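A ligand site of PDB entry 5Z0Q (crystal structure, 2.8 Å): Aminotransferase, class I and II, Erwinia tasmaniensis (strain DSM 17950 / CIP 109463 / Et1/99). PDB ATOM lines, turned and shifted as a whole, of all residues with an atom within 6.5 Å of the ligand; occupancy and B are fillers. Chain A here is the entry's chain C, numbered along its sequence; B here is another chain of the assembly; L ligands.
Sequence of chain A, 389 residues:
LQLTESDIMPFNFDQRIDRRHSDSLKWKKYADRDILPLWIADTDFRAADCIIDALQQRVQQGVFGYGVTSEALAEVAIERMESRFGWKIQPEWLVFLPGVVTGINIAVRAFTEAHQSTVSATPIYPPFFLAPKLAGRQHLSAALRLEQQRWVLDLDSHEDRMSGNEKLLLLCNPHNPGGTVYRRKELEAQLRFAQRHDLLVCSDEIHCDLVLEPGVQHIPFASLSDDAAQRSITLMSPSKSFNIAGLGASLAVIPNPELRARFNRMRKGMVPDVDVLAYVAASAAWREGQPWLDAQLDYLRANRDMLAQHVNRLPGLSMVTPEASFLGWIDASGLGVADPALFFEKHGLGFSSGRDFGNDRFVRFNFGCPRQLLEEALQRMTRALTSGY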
ATOM      1  N   ALA A  41       6.391  36.732 -14.008  1.00  0.00           N
ATOM      2  CA  ALA A  41       6.008  36.196 -12.707  1.00  0.00           C
ATOM      3  C   ALA A  41       7.244  36.070 -11.800  1.00  0.00           C
ATOM      4  O   ALA A  41       7.773  34.988 -11.538  1.00  0.00           O
ATOM      5  CB  ALA A  41       5.307  34.859 -12.875  1.00  0.00           C
ATOM      6  N   PRO A  98      17.222  22.016 -13.948  1.00  0.00           N
ATOM      7  CA  PRO A  98      17.485  23.467 -13.962  1.00  0.00           C
ATOM      8  C   PRO A  98      16.284  24.267 -14.467  1.00  0.00           C
ATOM      9  O   PRO A  98      16.302  24.915 -15.527  1.00  0.00           O
ATOM     10  CB  PRO A  98      18.690  23.574 -14.896  1.00  0.00           C
ATOM     11  CG  PRO A  98      18.458  22.473 -15.887  1.00  0.00           C
ATOM     12  CD  PRO A  98      17.794  21.341 -15.127  1.00  0.00           C
ATOM     13  N   GLY A  99      15.204  24.234 -13.699  1.00  0.00           N
ATOM     14  CA  GLY A  99      13.976  24.928 -14.045  1.00  0.00           C
ATOM     15  C   GLY A  99      12.783  23.979 -14.056  1.00  0.00           C
ATOM     16  O   GLY A  99      12.900  22.764 -13.930  1.00  0.00           O
ATOM     17  N   VAL A 100      11.611  24.592 -14.215  1.00  0.00           N
ATOM     18  CA  VAL A 100      10.348  23.851 -14.226  1.00  0.00           C
ATOM     19  C   VAL A 100       9.877  23.678 -15.657  1.00  0.00           C
ATOM     20  O   VAL A 100       9.270  22.658 -16.005  1.00  0.00           O
ATOM     21  CB  VAL A 100       9.287  24.557 -13.368  1.00  0.00           C
ATOM     22  CG1 VAL A 100       7.998  23.735 -13.330  1.00  0.00           C
ATOM     23  CG2 VAL A 100       9.813  24.795 -11.959  1.00  0.00           C
ATOM     24  N   VAL A 101      10.177  24.668 -16.510  1.00  0.00           N
ATOM     25  CA  VAL A 101       9.758  24.598 -17.901  1.00  0.00           C
ATOM     26  C   VAL A 101      10.404  23.411 -18.600  1.00  0.00           C
ATOM     27  O   VAL A 101       9.775  22.734 -19.422  1.00  0.00           O
ATOM     28  CB  VAL A 101      10.075  25.923 -18.625  1.00  0.00           C
ATOM     29  CG1 VAL A 101       9.688  25.849 -20.094  1.00  0.00           C
ATOM     30  CG2 VAL A 101       9.363  27.084 -17.944  1.00  0.00           C
ATOM     31  N   THR A 102      11.671  23.136 -18.283  1.00  0.00           N
ATOM     32  CA  THR A 102      12.337  21.980 -18.867  1.00  0.00           C
ATOM     33  C   THR A 102      11.696  20.679 -18.399  1.00  0.00           C
ATOM     34  O   THR A 102      11.650  19.706 -19.166  1.00  0.00           O
ATOM     35  CB  THR A 102      13.836  21.994 -18.525  1.00  0.00           C
ATOM     36  OG1 THR A 102      14.458  20.822 -19.064  1.00  0.00           O
ATOM     37  CG2 THR A 102      14.049  22.039 -17.017  1.00  0.00           C
ATOM     38  N   ILE A 104       8.515  20.283 -17.847  1.00  0.00           N
ATOM     39  CA  ILE A 104       7.299  20.138 -18.632  1.00  0.00           C
ATOM     40  C   ILE A 104       7.608  19.576 -20.011  1.00  0.00           C
ATOM     41  O   ILE A 104       6.891  18.703 -20.521  1.00  0.00           O
ATOM     42  CB  ILE A 104       6.555  21.484 -18.705  1.00  0.00           C
ATOM     43  CG1 ILE A 104       6.127  21.942 -17.316  1.00  0.00           C
ATOM     44  CG2 ILE A 104       5.354  21.387 -19.643  1.00  0.00           C
ATOM     45  CD1 ILE A 104       5.534  23.336 -17.278  1.00  0.00           C
ATOM     46  N   TYR A 125      -0.528  28.257 -17.929  1.00  0.00           N
ATOM     47  CA  TYR A 125       0.858  28.637 -18.156  1.00  0.00           C
ATOM     48  C   TYR A 125       1.245  28.320 -19.607  1.00  0.00           C
ATOM     49  O   TYR A 125       1.076  27.174 -20.054  1.00  0.00           O
ATOM     50  CB  TYR A 125       1.760  27.891 -17.167  1.00  0.00           C
ATOM     51  CG  TYR A 125       3.207  28.308 -17.143  1.00  0.00           C
ATOM     52  CD1 TYR A 125       3.566  29.645 -17.079  1.00  0.00           C
ATOM     53  CD2 TYR A 125       4.223  27.354 -17.138  1.00  0.00           C
ATOM     54  CE1 TYR A 125       4.895  30.025 -17.047  1.00  0.00           C
ATOM     55  CE2 TYR A 125       5.553  27.721 -17.101  1.00  0.00           C
ATOM     56  CZ  TYR A 125       5.883  29.058 -17.050  1.00  0.00           C
ATOM     57  OH  TYR A 125       7.212  29.434 -17.009  1.00  0.00           O
ATOM     58  N   PHE A 128       2.512  25.045 -21.264  1.00  0.00           N
ATOM     59  CA  PHE A 128       1.738  23.818 -21.157  1.00  0.00           C
ATOM     60  C   PHE A 128       1.225  23.364 -22.519  1.00  0.00           C
ATOM     61  O   PHE A 128       1.195  22.155 -22.808  1.00  0.00           O
ATOM     62  CB  PHE A 128       0.580  24.004 -20.188  1.00  0.00           C
ATOM     63  CG  PHE A 128       0.935  23.696 -18.772  1.00  0.00           C
ATOM     64  CD1 PHE A 128       1.733  24.565 -18.037  1.00  0.00           C
ATOM     65  CD2 PHE A 128       0.491  22.533 -18.172  1.00  0.00           C
ATOM     66  CE1 PHE A 128       2.070  24.280 -16.733  1.00  0.00           C
ATOM     67  CE2 PHE A 128       0.827  22.243 -16.859  1.00  0.00           C
ATOM     68  CZ  PHE A 128       1.618  23.110 -16.148  1.00  0.00           C
ATOM     69  N   CYS A 172      -2.098  21.928 -13.167  1.00  0.00           N
ATOM     70  CA  CYS A 172      -1.399  23.070 -12.570  1.00  0.00           C
ATOM     71  C   CYS A 172      -2.127  23.434 -11.280  1.00  0.00           C
ATOM     72  O   CYS A 172      -3.217  24.001 -11.321  1.00  0.00           O
ATOM     73  CB  CYS A 172      -1.363  24.249 -13.546  1.00  0.00           C
ATOM     74  SG  CYS A 172      -0.402  25.666 -12.982  1.00  0.00           S
ATOM     75  N   PRO A 174      -1.171  25.103  -7.399  1.00  0.00           N
ATOM     76  CA  PRO A 174      -2.168  26.124  -7.757  1.00  0.00           C
ATOM     77  C   PRO A 174      -2.074  26.550  -9.217  1.00  0.00           C
ATOM     78  O   PRO A 174      -1.018  26.441  -9.820  1.00  0.00           O
ATOM     79  CB  PRO A 174      -1.815  27.300  -6.832  1.00  0.00           C
ATOM     80  CG  PRO A 174      -1.011  26.706  -5.728  1.00  0.00           C
ATOM     81  CD  PRO A 174      -0.240  25.596  -6.371  1.00  0.00           C
ATOM     82  N   HIS A 175      -3.192  27.023  -9.774  1.00  0.00           N
ATOM     83  CA  HIS A 175      -3.305  27.221 -11.209  1.00  0.00           C
ATOM     84  C   HIS A 175      -2.805  28.602 -11.620  1.00  0.00           C
ATOM     85  O   HIS A 175      -3.260  29.614 -11.095  1.00  0.00           O
ATOM     86  CB  HIS A 175      -4.755  27.031 -11.660  1.00  0.00           C
ATOM     87  CG  HIS A 175      -4.928  27.114 -13.140  1.00  0.00           C
ATOM     88  ND1 HIS A 175      -4.997  28.311 -13.819  1.00  0.00           N
ATOM     89  CD2 HIS A 175      -5.043  26.144 -14.075  1.00  0.00           C
ATOM     90  CE1 HIS A 175      -5.142  28.075 -15.110  1.00  0.00           C
ATOM     91  NE2 HIS A 175      -5.182  26.762 -15.292  1.00  0.00           N
ATOM     92  N   ASN A 176      -1.873  28.624 -12.558  1.00  0.00           N
ATOM     93  CA  ASN A 176      -1.432  29.827 -13.250  1.00  0.00           C
ATOM     94  C   ASN A 176      -2.217  29.955 -14.549  1.00  0.00           C
ATOM     95  O   ASN A 176      -2.231  29.015 -15.353  1.00  0.00           O
ATOM     96  CB  ASN A 176       0.067  29.752 -13.550  1.00  0.00           C
ATOM     97  CG  ASN A 176       0.641  31.077 -14.002  1.00  0.00           C
ATOM     98  OD1 ASN A 176       0.236  32.142 -13.526  1.00  0.00           O
ATOM     99  ND2 ASN A 176       1.593  31.021 -14.929  1.00  0.00           N
ATOM    100  N   ASP A 204       2.073  20.580 -12.092  1.00  0.00           N
ATOM    101  CA  ASP A 204       2.976  21.700 -11.841  1.00  0.00           C
ATOM    102  C   ASP A 204       2.562  22.366 -10.545  1.00  0.00           C
ATOM    103  O   ASP A 204       1.507  23.017 -10.480  1.00  0.00           O
ATOM    104  CB  ASP A 204       2.952  22.684 -13.007  1.00  0.00           C
ATOM    105  CG  ASP A 204       4.082  23.694 -12.963  1.00  0.00           C
ATOM    106  OD1 ASP A 204       4.459  24.130 -11.850  1.00  0.00           O
ATOM    107  OD2 ASP A 204       4.598  24.057 -14.034  1.00  0.00           O
ATOM    108  N   ILE A 206       4.451  24.668  -8.581  1.00  0.00           N
ATOM    109  CA  ILE A 206       5.473  25.655  -8.249  1.00  0.00           C
ATOM    110  C   ILE A 206       4.950  26.665  -7.236  1.00  0.00           C
ATOM    111  O   ILE A 206       5.724  27.170  -6.412  1.00  0.00           O
ATOM    112  CB  ILE A 206       5.966  26.340  -9.540  1.00  0.00           C
ATOM    113  CG1 ILE A 206       6.982  27.452  -9.218  1.00  0.00           C
ATOM    114  CG2 ILE A 206       4.804  26.913 -10.320  1.00  0.00           C
ATOM    115  CD1 ILE A 206       8.245  26.948  -8.576  1.00  0.00           C
ATOM    116  N   HIS A 207       3.659  26.960  -7.249  1.00  0.00           N
ATOM    117  CA  HIS A 207       3.064  27.936  -6.344  1.00  0.00           C
ATOM    118  C   HIS A 207       2.531  27.322  -5.057  1.00  0.00           C
ATOM    119  O   HIS A 207       1.781  27.982  -4.338  1.00  0.00           O
ATOM    120  CB  HIS A 207       1.930  28.683  -7.055  1.00  0.00           C
ATOM    121  CG  HIS A 207       2.375  29.515  -8.219  1.00  0.00           C
ATOM    122  ND1 HIS A 207       2.469  29.011  -9.500  1.00  0.00           N
ATOM    123  CD2 HIS A 207       2.781  30.800  -8.295  1.00  0.00           C
ATOM    124  CE1 HIS A 207       2.891  29.952 -10.311  1.00  0.00           C
ATOM    125  NE2 HIS A 207       3.090  31.059  -9.604  1.00  0.00           N
ATOM    126  N   SER A 237       9.557  23.540  -6.820  1.00  0.00           N
ATOM    127  CA  SER A 237      10.738  24.377  -6.761  1.00  0.00           C
ATOM    128  C   SER A 237      10.507  25.565  -5.822  1.00  0.00           C
ATOM    129  O   SER A 237       9.374  26.016  -5.665  1.00  0.00           O
ATOM    130  CB  SER A 237      11.107  24.883  -8.154  1.00  0.00           C
ATOM    131  OG  SER A 237      12.081  25.901  -8.096  1.00  0.00           O
ATOM    132  N   SER A 239      11.635  28.450  -6.512  1.00  0.00           N
ATOM    133  CA  SER A 239      12.009  29.567  -7.368  1.00  0.00           C
ATOM    134  C   SER A 239      11.068  30.749  -7.178  1.00  0.00           C
ATOM    135  O   SER A 239      11.508  31.883  -6.989  1.00  0.00           O
ATOM    136  CB  SER A 239      12.028  29.128  -8.835  1.00  0.00           C
ATOM    137  OG  SER A 239      13.083  28.210  -9.074  1.00  0.00           O
ATOM    138  N   LYS A 240       9.760  30.503  -7.203  1.00  0.00           N
ATOM    139  CA  LYS A 240       8.788  31.576  -7.053  1.00  0.00           C
ATOM    140  C   LYS A 240       8.456  31.856  -5.593  1.00  0.00           C
ATOM    141  O   LYS A 240       8.073  32.991  -5.270  1.00  0.00           O
ATOM    142  CB  LYS A 240       7.503  31.243  -7.817  1.00  0.00           C
ATOM    143  CG  LYS A 240       7.724  31.048  -9.292  1.00  0.00           C
ATOM    144  CD  LYS A 240       6.411  30.979 -10.039  1.00  0.00           C
ATOM    145  CE  LYS A 240       6.428  31.917 -11.234  1.00  0.00           C
ATOM    146  NZ  LYS A 240       7.561  31.636 -12.148  1.00  0.00           N
ATOM    147  N   ALA A 245      14.078  32.502  -9.158  1.00  0.00           N
ATOM    148  CA  ALA A 245      13.914  31.909 -10.478  1.00  0.00           C
ATOM    149  C   ALA A 245      15.104  32.179 -11.385  1.00  0.00           C
ATOM    150  O   ALA A 245      15.329  31.414 -12.333  1.00  0.00           O
ATOM    151  CB  ALA A 245      12.629  32.437 -11.133  1.00  0.00           C
ATOM    152  N   GLY A 248      17.061  28.963 -10.733  1.00  0.00           N
ATOM    153  CA  GLY A 248      16.318  27.903 -11.384  1.00  0.00           C
ATOM    154  C   GLY A 248      16.585  26.494 -10.894  1.00  0.00           C
ATOM    155  O   GLY A 248      16.712  25.576 -11.710  1.00  0.00           O
ATOM    156  N   ALA A 249      16.676  26.291  -9.583  1.00  0.00           N
ATOM    157  CA  ALA A 249      16.840  24.964  -9.020  1.00  0.00           C
ATOM    158  C   ALA A 249      15.459  24.373  -8.766  1.00  0.00           C
ATOM    159  O   ALA A 249      14.673  24.934  -7.984  1.00  0.00           O
ATOM    160  CB  ALA A 249      17.665  25.006  -7.741  1.00  0.00           C
ATOM    161  N   SER A 250      15.151  23.252  -9.410  1.00  0.00           N
ATOM    162  CA  SER A 250      13.858  22.605  -9.294  1.00  0.00           C
ATOM    163  C   SER A 250      14.066  21.099  -9.170  1.00  0.00           C
ATOM    164  O   SER A 250      15.187  20.596  -9.263  1.00  0.00           O
ATOM    165  CB  SER A 250      12.960  22.933 -10.491  1.00  0.00           C
ATOM    166  OG  SER A 250      13.461  22.335 -11.674  1.00  0.00           O
ATOM    167  N   LEU A 327      -0.674  36.533  -8.490  1.00  0.00           N
ATOM    168  CA  LEU A 327      -1.381  37.013  -9.670  1.00  0.00           C
ATOM    169  C   LEU A 327      -2.776  36.385  -9.642  1.00  0.00           C
ATOM    170  O   LEU A 327      -2.943  35.262  -9.167  1.00  0.00           O
ATOM    171  CB  LEU A 327      -0.642  36.655 -10.969  1.00  0.00           C
ATOM    172  CG  LEU A 327       0.899  36.682 -10.946  1.00  0.00           C
ATOM    173  CD1 LEU A 327       1.466  35.270 -10.851  1.00  0.00           C
ATOM    174  CD2 LEU A 327       1.472  37.429 -12.138  1.00  0.00           C
ATOM    175  N   ARG A 364      -2.823  39.671 -16.940  1.00  0.00           N
ATOM    176  CA  ARG A 364      -2.301  39.139 -15.698  1.00  0.00           C
ATOM    177  C   ARG A 364      -1.615  40.250 -14.908  1.00  0.00           C
ATOM    178  O   ARG A 364      -0.729  40.937 -15.433  1.00  0.00           O
ATOM    179  CB  ARG A 364      -1.336  37.984 -15.940  1.00  0.00           C
ATOM    180  CG  ARG A 364      -1.119  37.091 -14.719  1.00  0.00           C
ATOM    181  CD  ARG A 364      -0.206  35.926 -15.013  1.00  0.00           C
ATOM    182  NE  ARG A 364       1.174  36.351 -15.243  1.00  0.00           N
ATOM    183  CZ  ARG A 364       2.207  35.520 -15.335  1.00  0.00           C
ATOM    184  NH1 ARG A 364       2.021  34.212 -15.208  1.00  0.00           N
ATOM    185  NH2 ARG A 364       3.425  35.997 -15.554  1.00  0.00           N
ATOM    186  N   TYR B  66      14.210  36.658 -12.871  1.00  0.00           N
ATOM    187  CA  TYR B  66      14.587  36.322 -14.232  1.00  0.00           C
ATOM    188  C   TYR B  66      15.525  37.369 -14.823  1.00  0.00           C
ATOM    189  O   TYR B  66      15.318  38.576 -14.663  1.00  0.00           O
ATOM    190  CB  TYR B  66      13.332  36.190 -15.113  1.00  0.00           C
ATOM    191  CG  TYR B  66      12.454  35.011 -14.752  1.00  0.00           C
ATOM    192  CD1 TYR B  66      12.779  33.727 -15.168  1.00  0.00           C
ATOM    193  CD2 TYR B  66      11.306  35.189 -13.994  1.00  0.00           C
ATOM    194  CE1 TYR B  66      11.973  32.654 -14.841  1.00  0.00           C
ATOM    195  CE2 TYR B  66      10.500  34.113 -13.659  1.00  0.00           C
ATOM    196  CZ  TYR B  66      10.843  32.848 -14.085  1.00  0.00           C
ATOM    197  OH  TYR B  66      10.048  31.777 -13.758  1.00  0.00           O
ATOM    198  N   PRO B 272      17.213  25.358 -20.691  1.00  0.00           N
ATOM    199  CA  PRO B 272      16.823  26.640 -20.095  1.00  0.00           C
ATOM    200  C   PRO B 272      17.849  27.729 -20.409  1.00  0.00           C
ATOM    201  O   PRO B 272      18.858  27.502 -21.068  1.00  0.00           O
ATOM    202  CB  PRO B 272      16.782  26.323 -18.605  1.00  0.00           C
ATOM    203  CG  PRO B 272      17.847  25.286 -18.435  1.00  0.00           C
ATOM    204  CD  PRO B 272      17.820  24.452 -19.698  1.00  0.00           C
HETATM  205  N1  LIG L   1       5.508  26.853 -13.716  1.00  0.00           N
HETATM  206  C1  LIG L   1       4.548  27.841 -13.570  1.00  0.00           C
HETATM  207  C2  LIG L   1       3.090  27.482 -13.580  1.00  0.00           C
HETATM  208  C3  LIG L   1       4.933  29.170 -13.398  1.00  0.00           C
HETATM  209  O1  LIG L   1       3.985  30.146 -13.245  1.00  0.00           O
HETATM  210  C4  LIG L   1       6.282  29.493 -13.379  1.00  0.00           C
HETATM  211  C5  LIG L   1       6.714  30.897 -13.027  1.00  0.00           C
HETATM  212  C6  LIG L   1       7.245  28.500 -13.538  1.00  0.00           C
HETATM  213  C7  LIG L   1       6.847  27.179 -13.708  1.00  0.00           C
HETATM  214  C8  LIG L   1       8.708  28.878 -13.519  1.00  0.00           C
HETATM  215  O2  LIG L   1       9.485  27.903 -14.189  1.00  0.00           O
HETATM  216  P1  LIG L   1      11.026  28.233 -14.536  1.00  0.00           P
HETATM  217  O3  LIG L   1      11.109  29.581 -15.214  1.00  0.00           O
HETATM  218  O4  LIG L   1      11.575  27.168 -15.462  1.00  0.00           O
HETATM  219  O5  LIG L   1      11.813  28.257 -13.257  1.00  0.00           O
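A carbon (C5) of the ligand is bonded to the side-chain amino group (NZ) of Lys 240, at 1.4 Å. OH of Tyr 66 of chain B lies within hydrogen-bond range of O3 of the ligand (2.8 Å). The backbone NH (N) of Val 100 is in hydrogen-bond range of an oxygen (O4) of the ligand, at 2.9 Å. The backbone NH of Val 101 lies within hydrogen-bond range of an oxygen (O4) of the ligand (3.1 Å). The side-chain amide nitrogen (ND2) of Asn 176 sits at hydrogen-bond distance from an oxygen (O1) of the ligand (3.1 Å).
OD2 of Asp 204 sits close to N1 of the ligand. Residues that only touch the ligand: Gly 99 (3.6 Å), Tyr 125 (3.5 Å), Cys 172 (3.98 Å), Ile 206 (3.4 Å) and His 207 (3.1 Å). Hydrophobic or aromatic side chains that line the ligand: Val 100, Val 101, Tyr 125, Ile 206, His 207 and Tyr 66 of chain B. Of the 27 residues printed, 11 come within 4 Å of the ligand.
NZ of Lys 240 is in hydrogen-bond range of OH of Tyr 66 of chain B, at 3.0 Å. OD1 of Asp 204 sits close to N of Ile 206 (3.3 Å). The backbone carbonyl oxygen (O) of Asn 176 is in hydrogen-bond range of the backbone NH (N) of Tyr 125 (3.2 Å). N of Asn 176 is in hydrogen-bond range of SG of Cys 172, 3.3 Å away. The side-chain amide oxygen (OD1) of Asn 176 sits at hydrogen-bond distance from the guanidinium group (NH1) of Arg 364. The backbone NH (N) of Gly 99 lies within hydrogen-bond range of the backbone carbonyl oxygen (O) of Gly 248. The backbone NH (N) of Gly 99 lies close to the side-chain hydroxyl (OG) of Ser 250 (3.3 Å). SG of Cys 172 sits at hydrogen-bond distance from O of Pro 174 (3.3 Å).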
